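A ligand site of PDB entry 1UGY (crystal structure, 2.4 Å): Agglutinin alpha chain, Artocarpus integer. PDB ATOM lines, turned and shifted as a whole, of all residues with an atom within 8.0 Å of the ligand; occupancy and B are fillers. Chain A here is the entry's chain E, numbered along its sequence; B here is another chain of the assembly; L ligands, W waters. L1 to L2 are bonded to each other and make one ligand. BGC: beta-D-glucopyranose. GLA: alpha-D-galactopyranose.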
ATOM      1  N   GLY A   1      10.809  22.309  14.997  1.00  0.00           N
ATOM      2  CA  GLY A   1      10.598  20.851  14.846  1.00  0.00           C
ATOM      3  C   GLY A   1      10.504  20.144  16.184  1.00  0.00           C
ATOM      4  O   GLY A   1      10.569  20.799  17.231  1.00  0.00           O
ATOM      5  N   LYS A   2      10.371  18.823  16.162  1.00  0.00           N
ATOM      6  CA  LYS A   2      10.279  18.036  17.391  1.00  0.00           C
ATOM      7  C   LYS A   2      11.676  17.664  17.889  1.00  0.00           C
ATOM      8  O   LYS A   2      12.465  17.088  17.153  1.00  0.00           O
ATOM      9  CB  LYS A   2       9.453  16.773  17.142  1.00  0.00           C
ATOM     10  CG  LYS A   2       9.249  15.919  18.380  1.00  0.00           C
ATOM     11  CD  LYS A   2       8.594  14.590  18.049  1.00  0.00           C
ATOM     12  CE  LYS A   2       8.472  13.721  19.299  1.00  0.00           C
ATOM     13  NZ  LYS A   2       7.933  12.363  18.979  1.00  0.00           N
ATOM     14  N   ALA A  24      17.447  19.466   2.494  1.00  0.00           N
ATOM     15  CA  ALA A  24      18.407  19.179   3.544  1.00  0.00           C
ATOM     16  C   ALA A  24      18.251  17.746   4.050  1.00  0.00           C
ATOM     17  O   ALA A  24      17.624  16.907   3.390  1.00  0.00           O
ATOM     18  CB  ALA A  24      18.212  20.154   4.692  1.00  0.00           C
ATOM     19  N   ILE A  25      18.832  17.470   5.220  1.00  0.00           N
ATOM     20  CA  ILE A  25      18.758  16.158   5.840  1.00  0.00           C
ATOM     21  C   ILE A  25      17.370  15.937   6.437  1.00  0.00           C
ATOM     22  O   ILE A  25      16.777  16.864   7.007  1.00  0.00           O
ATOM     23  CB  ILE A  25      19.815  16.007   6.963  1.00  0.00           C
ATOM     24  CG1 ILE A  25      21.228  16.190   6.402  1.00  0.00           C
ATOM     25  CG2 ILE A  25      19.684  14.637   7.625  1.00  0.00           C
ATOM     26  CD1 ILE A  25      21.619  15.179   5.343  1.00  0.00           C
ATOM     27  N   SER A  46      11.282  12.937   9.702  1.00  0.00           N
ATOM     28  CA  SER A  46      10.825  14.221   9.201  1.00  0.00           C
ATOM     29  C   SER A  46       9.301  14.217   9.115  1.00  0.00           C
ATOM     30  O   SER A  46       8.690  13.158   8.937  1.00  0.00           O
ATOM     31  CB  SER A  46      11.403  14.468   7.813  1.00  0.00           C
ATOM     32  OG  SER A  46      10.705  15.494   7.151  1.00  0.00           O
ATOM     33  N   PHE A  47       8.689  15.390   9.228  1.00  0.00           N
ATOM     34  CA  PHE A  47       7.237  15.476   9.136  1.00  0.00           C
ATOM     35  C   PHE A  47       6.739  15.125   7.735  1.00  0.00           C
ATOM     36  O   PHE A  47       5.547  14.939   7.523  1.00  0.00           O
ATOM     37  CB  PHE A  47       6.744  16.887   9.501  1.00  0.00           C
ATOM     38  CG  PHE A  47       7.008  17.303  10.920  1.00  0.00           C
ATOM     39  CD1 PHE A  47       7.303  16.360  11.908  1.00  0.00           C
ATOM     40  CD2 PHE A  47       6.930  18.647  11.287  1.00  0.00           C
ATOM     41  CE1 PHE A  47       7.519  16.743  13.240  1.00  0.00           C
ATOM     42  CE2 PHE A  47       7.145  19.050  12.604  1.00  0.00           C
ATOM     43  CZ  PHE A  47       7.434  18.092  13.586  1.00  0.00           C
ATOM     44  N   ILE A  48       7.662  15.037   6.778  1.00  0.00           N
ATOM     45  CA  ILE A  48       7.294  14.714   5.396  1.00  0.00           C
ATOM     46  C   ILE A  48       8.148  13.564   4.856  1.00  0.00           C
ATOM     47  O   ILE A  48       8.871  12.928   5.608  1.00  0.00           O
ATOM     48  CB  ILE A  48       7.470  15.939   4.465  1.00  0.00           C
ATOM     49  CG1 ILE A  48       8.897  16.476   4.570  1.00  0.00           C
ATOM     50  CG2 ILE A  48       6.474  17.014   4.845  1.00  0.00           C
ATOM     51  CD1 ILE A  48       9.254  17.494   3.513  1.00  0.00           C
ATOM     52  N   VAL A  75      16.569  27.322   4.248  1.00  0.00           N
ATOM     53  CA  VAL A  75      15.687  26.549   3.401  1.00  0.00           C
ATOM     54  C   VAL A  75      14.285  26.923   3.861  1.00  0.00           C
ATOM     55  O   VAL A  75      13.929  26.712   5.021  1.00  0.00           O
ATOM     56  CB  VAL A  75      15.911  25.027   3.535  1.00  0.00           C
ATOM     57  CG1 VAL A  75      14.866  24.287   2.741  1.00  0.00           C
ATOM     58  CG2 VAL A  75      17.286  24.659   3.018  1.00  0.00           C
ATOM     59  N   SER A  76      13.508  27.503   2.952  1.00  0.00           N
ATOM     60  CA  SER A  76      12.148  27.932   3.240  1.00  0.00           C
ATOM     61  C   SER A  76      12.066  28.883   4.441  1.00  0.00           C
ATOM     62  O   SER A  76      11.071  28.884   5.167  1.00  0.00           O
ATOM     63  CB  SER A  76      11.257  26.718   3.498  1.00  0.00           C
ATOM     64  OG  SER A  76       9.902  27.112   3.642  1.00  0.00           O
ATOM     65  N   GLY A  77      13.087  29.693   4.644  1.00  0.00           N
ATOM     66  CA  GLY A  77      13.062  30.636   5.746  1.00  0.00           C
ATOM     67  C   GLY A  77      13.536  30.094   7.088  1.00  0.00           C
ATOM     68  O   GLY A  77      13.512  30.816   8.083  1.00  0.00           O
ATOM     69  N   TYR A  78      13.970  28.844   7.106  1.00  0.00           N
ATOM     70  CA  TYR A  78      14.456  28.222   8.329  1.00  0.00           C
ATOM     71  C   TYR A  78      15.933  27.893   8.167  1.00  0.00           C
ATOM     72  O   TYR A  78      16.401  27.694   7.054  1.00  0.00           O
ATOM     73  CB  TYR A  78      13.730  26.897   8.594  1.00  0.00           C
ATOM     74  CG  TYR A  78      12.231  27.008   8.721  1.00  0.00           C
ATOM     75  CD1 TYR A  78      11.639  27.496   9.892  1.00  0.00           C
ATOM     76  CD2 TYR A  78      11.393  26.613   7.674  1.00  0.00           C
ATOM     77  CE1 TYR A  78      10.261  27.574  10.014  1.00  0.00           C
ATOM     78  CE2 TYR A  78      10.009  26.691   7.789  1.00  0.00           C
ATOM     79  CZ  TYR A  78       9.451  27.178   8.957  1.00  0.00           C
ATOM     80  OH  TYR A  78       8.079  27.257   9.087  1.00  0.00           O
ATOM     81  N   VAL A  79      16.673  27.847   9.268  1.00  0.00           N
ATOM     82  CA  VAL A  79      18.075  27.476   9.200  1.00  0.00           C
ATOM     83  C   VAL A  79      18.123  26.006   9.580  1.00  0.00           C
ATOM     84  O   VAL A  79      17.620  25.613  10.635  1.00  0.00           O
ATOM     85  CB  VAL A  79      18.939  28.281  10.176  1.00  0.00           C
ATOM     86  CG1 VAL A  79      20.409  27.862  10.031  1.00  0.00           C
ATOM     87  CG2 VAL A  79      18.762  29.777   9.915  1.00  0.00           C
ATOM     88  N   VAL A  80      18.715  25.183   8.723  1.00  0.00           N
ATOM     89  CA  VAL A  80      18.771  23.744   8.962  1.00  0.00           C
ATOM     90  C   VAL A  80      20.104  23.134   8.547  1.00  0.00           C
ATOM     91  O   VAL A  80      20.924  23.790   7.903  1.00  0.00           O
ATOM     92  CB  VAL A  80      17.645  23.027   8.167  1.00  0.00           C
ATOM     93  CG1 VAL A  80      16.300  23.548   8.616  1.00  0.00           C
ATOM     94  CG2 VAL A  80      17.809  23.261   6.669  1.00  0.00           C
ATOM     95  N   VAL A  81      20.326  21.879   8.913  1.00  0.00           N
ATOM     96  CA  VAL A  81      21.548  21.164   8.538  1.00  0.00           C
ATOM     97  C   VAL A  81      21.265  20.603   7.152  1.00  0.00           C
ATOM     98  O   VAL A  81      20.362  19.789   6.994  1.00  0.00           O
ATOM     99  CB  VAL A  81      21.842  20.005   9.514  1.00  0.00           C
ATOM    100  CG1 VAL A  81      23.133  19.301   9.131  1.00  0.00           C
ATOM    101  CG2 VAL A  81      21.942  20.554  10.936  1.00  0.00           C
ATOM    102  N   SER A 119      16.843  18.196  16.780  1.00  0.00           N
ATOM    103  CA  SER A 119      15.471  18.546  16.485  1.00  0.00           C
ATOM    104  C   SER A 119      15.205  18.336  15.006  1.00  0.00           C
ATOM    105  O   SER A 119      16.046  18.652  14.174  1.00  0.00           O
ATOM    106  CB  SER A 119      15.211  20.006  16.834  1.00  0.00           C
ATOM    107  OG  SER A 119      13.895  20.390  16.489  1.00  0.00           O
ATOM    108  N   ILE A 120      14.045  17.778  14.693  1.00  0.00           N
ATOM    109  CA  ILE A 120      13.679  17.540  13.299  1.00  0.00           C
ATOM    110  C   ILE A 120      12.228  17.944  13.077  1.00  0.00           C
ATOM    111  O   ILE A 120      11.331  17.538  13.822  1.00  0.00           O
ATOM    112  CB  ILE A 120      13.831  16.048  12.913  1.00  0.00           C
ATOM    113  CG1 ILE A 120      15.270  15.590  13.152  1.00  0.00           C
ATOM    114  CG2 ILE A 120      13.468  15.852  11.460  1.00  0.00           C
ATOM    115  CD1 ILE A 120      15.473  14.104  12.972  1.00  0.00           C
ATOM    116  N   GLY A 121      12.009  18.790  12.076  1.00  0.00           N
ATOM    117  CA  GLY A 121      10.682  19.228  11.708  1.00  0.00           C
ATOM    118  C   GLY A 121      10.582  18.674  10.298  1.00  0.00           C
ATOM    119  O   GLY A 121      10.516  17.459  10.116  1.00  0.00           O
ATOM    120  N   TYR A 122      10.561  19.552   9.298  1.00  0.00           N
ATOM    121  CA  TYR A 122      10.542  19.059   7.932  1.00  0.00           C
ATOM    122  C   TYR A 122      11.943  18.516   7.701  1.00  0.00           C
ATOM    123  O   TYR A 122      12.132  17.499   7.034  1.00  0.00           O
ATOM    124  CB  TYR A 122      10.283  20.203   6.955  1.00  0.00           C
ATOM    125  CG  TYR A 122       8.844  20.301   6.485  1.00  0.00           C
ATOM    126  CD1 TYR A 122       8.550  20.747   5.200  1.00  0.00           C
ATOM    127  CD2 TYR A 122       7.787  19.927   7.320  1.00  0.00           C
ATOM    128  CE1 TYR A 122       7.240  20.831   4.754  1.00  0.00           C
ATOM    129  CE2 TYR A 122       6.476  19.997   6.876  1.00  0.00           C
ATOM    130  CZ  TYR A 122       6.206  20.457   5.596  1.00  0.00           C
ATOM    131  OH  TYR A 122       4.908  20.563   5.151  1.00  0.00           O
ATOM    132  N   TRP A 123      12.925  19.207   8.279  1.00  0.00           N
ATOM    133  CA  TRP A 123      14.321  18.820   8.151  1.00  0.00           C
ATOM    134  C   TRP A 123      15.020  18.875   9.510  1.00  0.00           C
ATOM    135  O   TRP A 123      14.430  19.317  10.501  1.00  0.00           O
ATOM    136  CB  TRP A 123      15.023  19.763   7.180  1.00  0.00           C
ATOM    137  CG  TRP A 123      14.354  19.833   5.847  1.00  0.00           C
ATOM    138  CD1 TRP A 123      14.365  18.872   4.877  1.00  0.00           C
ATOM    139  CD2 TRP A 123      13.514  20.887   5.366  1.00  0.00           C
ATOM    140  NE1 TRP A 123      13.583  19.268   3.823  1.00  0.00           N
ATOM    141  CE2 TRP A 123      13.048  20.497   4.100  1.00  0.00           C
ATOM    142  CE3 TRP A 123      13.108  22.117   5.890  1.00  0.00           C
ATOM    143  CZ2 TRP A 123      12.191  21.305   3.336  1.00  0.00           C
ATOM    144  CZ3 TRP A 123      12.251  22.920   5.138  1.00  0.00           C
ATOM    145  CH2 TRP A 123      11.807  22.508   3.869  1.00  0.00           C
ATOM    146  N   LEU A 124      16.257  18.400   9.539  1.00  0.00           N
ATOM    147  CA  LEU A 124      17.055  18.427  10.766  1.00  0.00           C
ATOM    148  C   LEU A 124      17.341  19.895  11.063  1.00  0.00           C
ATOM    149  O   LEU A 124      18.050  20.562  10.314  1.00  0.00           O
ATOM    150  CB  LEU A 124      18.368  17.652  10.545  1.00  0.00           C
ATOM    151  CG  LEU A 124      19.331  17.512  11.732  1.00  0.00           C
ATOM    152  CD1 LEU A 124      18.623  16.830  12.887  1.00  0.00           C
ATOM    153  CD2 LEU A 124      20.553  16.703  11.303  1.00  0.00           C
ATOM    154  N   ASP A 125      16.785  20.421  12.147  1.00  0.00           N
ATOM    155  CA  ASP A 125      16.985  21.825  12.484  1.00  0.00           C
ATOM    156  C   ASP A 125      18.365  22.076  13.094  1.00  0.00           C
ATOM    157  O   ASP A 125      19.013  23.082  12.788  1.00  0.00           O
ATOM    158  CB  ASP A 125      15.909  22.319  13.456  1.00  0.00           C
ATOM    159  CG  ASP A 125      14.507  22.061  12.944  1.00  0.00           C
ATOM    160  OD1 ASP A 125      14.206  22.485  11.811  1.00  0.00           O
ATOM    161  OD2 ASP A 125      13.722  21.430  13.673  1.00  0.00           O
ATOM    162  N   TYR A 126      18.791  21.162  13.956  1.00  0.00           N
ATOM    163  CA  TYR A 126      20.099  21.289  14.588  1.00  0.00           C
ATOM    164  C   TYR A 126      20.431  20.021  15.349  1.00  0.00           C
ATOM    165  O   TYR A 126      19.547  19.200  15.607  1.00  0.00           O
ATOM    166  CB  TYR A 126      20.101  22.497  15.545  1.00  0.00           C
ATOM    167  CG  TYR A 126      19.116  22.392  16.694  1.00  0.00           C
ATOM    168  CD1 TYR A 126      19.337  21.502  17.739  1.00  0.00           C
ATOM    169  CD2 TYR A 126      17.969  23.187  16.723  1.00  0.00           C
ATOM    170  CE1 TYR A 126      18.432  21.403  18.794  1.00  0.00           C
ATOM    171  CE2 TYR A 126      17.059  23.096  17.781  1.00  0.00           C
ATOM    172  CZ  TYR A 126      17.291  22.204  18.817  1.00  0.00           C
ATOM    173  OH  TYR A 126      16.422  22.113  19.881  1.00  0.00           O
ATOM    174  N   ALA B  17      19.991  25.744  13.427  1.00  0.00           N
ATOM    175  CA  ALA B  17      19.223  26.859  13.977  1.00  0.00           C
ATOM    176  C   ALA B  17      19.784  27.254  15.347  1.00  0.00           C
ATOM    177  O   ALA B  17      20.245  26.397  16.108  1.00  0.00           O
ATOM    178  CB  ALA B  17      17.754  26.475  14.099  1.00  0.00           C
HETATM  179  C2  BGC L   1       3.815  23.563   7.638  1.00  0.00           C
HETATM  180  C3  BGC L   1       4.552  24.822   7.163  1.00  0.00           C
HETATM  181  C4  BGC L   1       5.884  24.952   7.879  1.00  0.00           C
HETATM  182  C5  BGC L   1       6.657  23.674   7.644  1.00  0.00           C
HETATM  183  C6  BGC L   1       8.049  23.659   8.144  1.00  0.00           C
HETATM  184  C1  BGC L   1       4.713  22.316   7.661  1.00  0.00           C
HETATM  185  O1  BGC L   1       4.098  21.284   8.360  1.00  0.00           O
HETATM  186  O2  BGC L   1       2.689  23.309   6.789  1.00  0.00           O
HETATM  187  O3  BGC L   1       3.767  25.990   7.369  1.00  0.00           O
HETATM  188  O4  BGC L   1       6.584  26.070   7.348  1.00  0.00           O
HETATM  189  O5  BGC L   1       5.979  22.600   8.284  1.00  0.00           O
HETATM  190  O6  BGC L   1       8.074  23.846   9.567  1.00  0.00           O
HETATM  191  C1  GLA L   2       8.616  22.778  10.259  1.00  0.00           C
HETATM  192  C2  GLA L   2       8.579  23.108  11.730  1.00  0.00           C
HETATM  193  C3  GLA L   2       9.593  24.195  12.025  1.00  0.00           C
HETATM  194  C4  GLA L   2      10.987  23.735  11.569  1.00  0.00           C
HETATM  195  C5  GLA L   2      10.953  23.418  10.077  1.00  0.00           C
HETATM  196  C6  GLA L   2      12.258  22.979   9.443  1.00  0.00           C
HETATM  197  O2  GLA L   2       7.283  23.579  12.078  1.00  0.00           O
HETATM  198  O3  GLA L   2       9.581  24.536  13.422  1.00  0.00           O
HETATM  199  O4  GLA L   2      11.369  22.608  12.323  1.00  0.00           O
HETATM  200  O5  GLA L   2       9.938  22.421   9.811  1.00  0.00           O
HETATM  201  O6  GLA L   2      12.487  21.610   9.647  1.00  0.00           O
HETATM  202  O   HOH W   1       3.330  24.154  10.369  1.00  0.00           O
HETATM  203  O   HOH W   2       0.517  24.879   6.616  1.00  0.00           O
HETATM  204  O   HOH W   3       4.717  22.018  10.754  1.00  0.00           O
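O4 of BGC L1 lies within hydrogen-bond range of OH of Tyr 78 (2.6 Å). The backbone NH of Gly 1 lies within hydrogen-bond range of an oxygen (O4) of GLA L2 (2.7 Å). An oxygen (O6) of GLA L2 lies within hydrogen-bond range of the backbone NH of Trp 123, at 2.8 Å. The backbone carbonyl oxygen of Trp 123 sits at hydrogen-bond distance from an oxygen (O6) of GLA L2 (3.1 Å). An oxygen (O6) of GLA L2 lies within hydrogen-bond range of the backbone NH of Tyr 122 (2.8 Å). The side-chain hydroxyl (OH) of Tyr 122 lies close to an oxygen (O1) of BGC L1 (3.4 Å). OD1 of Asp 125 lies within hydrogen-bond range of O4 of GLA L2, at 2.9 Å.
N of Gly 1 sits at hydrogen-bond distance from OD2 of Asp 125 (3.3 Å). O of Gly 1 lies close to OG of Ser 119, 3.4 Å away. The side-chain hydroxyl of Ser 46 sits at hydrogen-bond distance from the backbone carbonyl oxygen of Tyr 122, at 2.5 Å. The backbone NH (N) of Asp 125 lies within hydrogen-bond range of the backbone carbonyl oxygen (O) of Ser 119 (2.8 Å). O of Asp 125 is in hydrogen-bond range of N of Ala 17 of chain B, 2.9 Å away. O of Gly 121 is in hydrogen-bond range of N of Phe 47, at 2.9 Å.
Residues that only touch the ligand: Gly 121 (3.5 Å). Hydrophobic or aromatic side chains within 4 Å of the ligand: Tyr 78, Tyr 122 and Trp 123. Within 4 Å of the ligand: Gly 1, Tyr 78, Gly 121, Tyr 122, Trp 123 and Asp 125.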
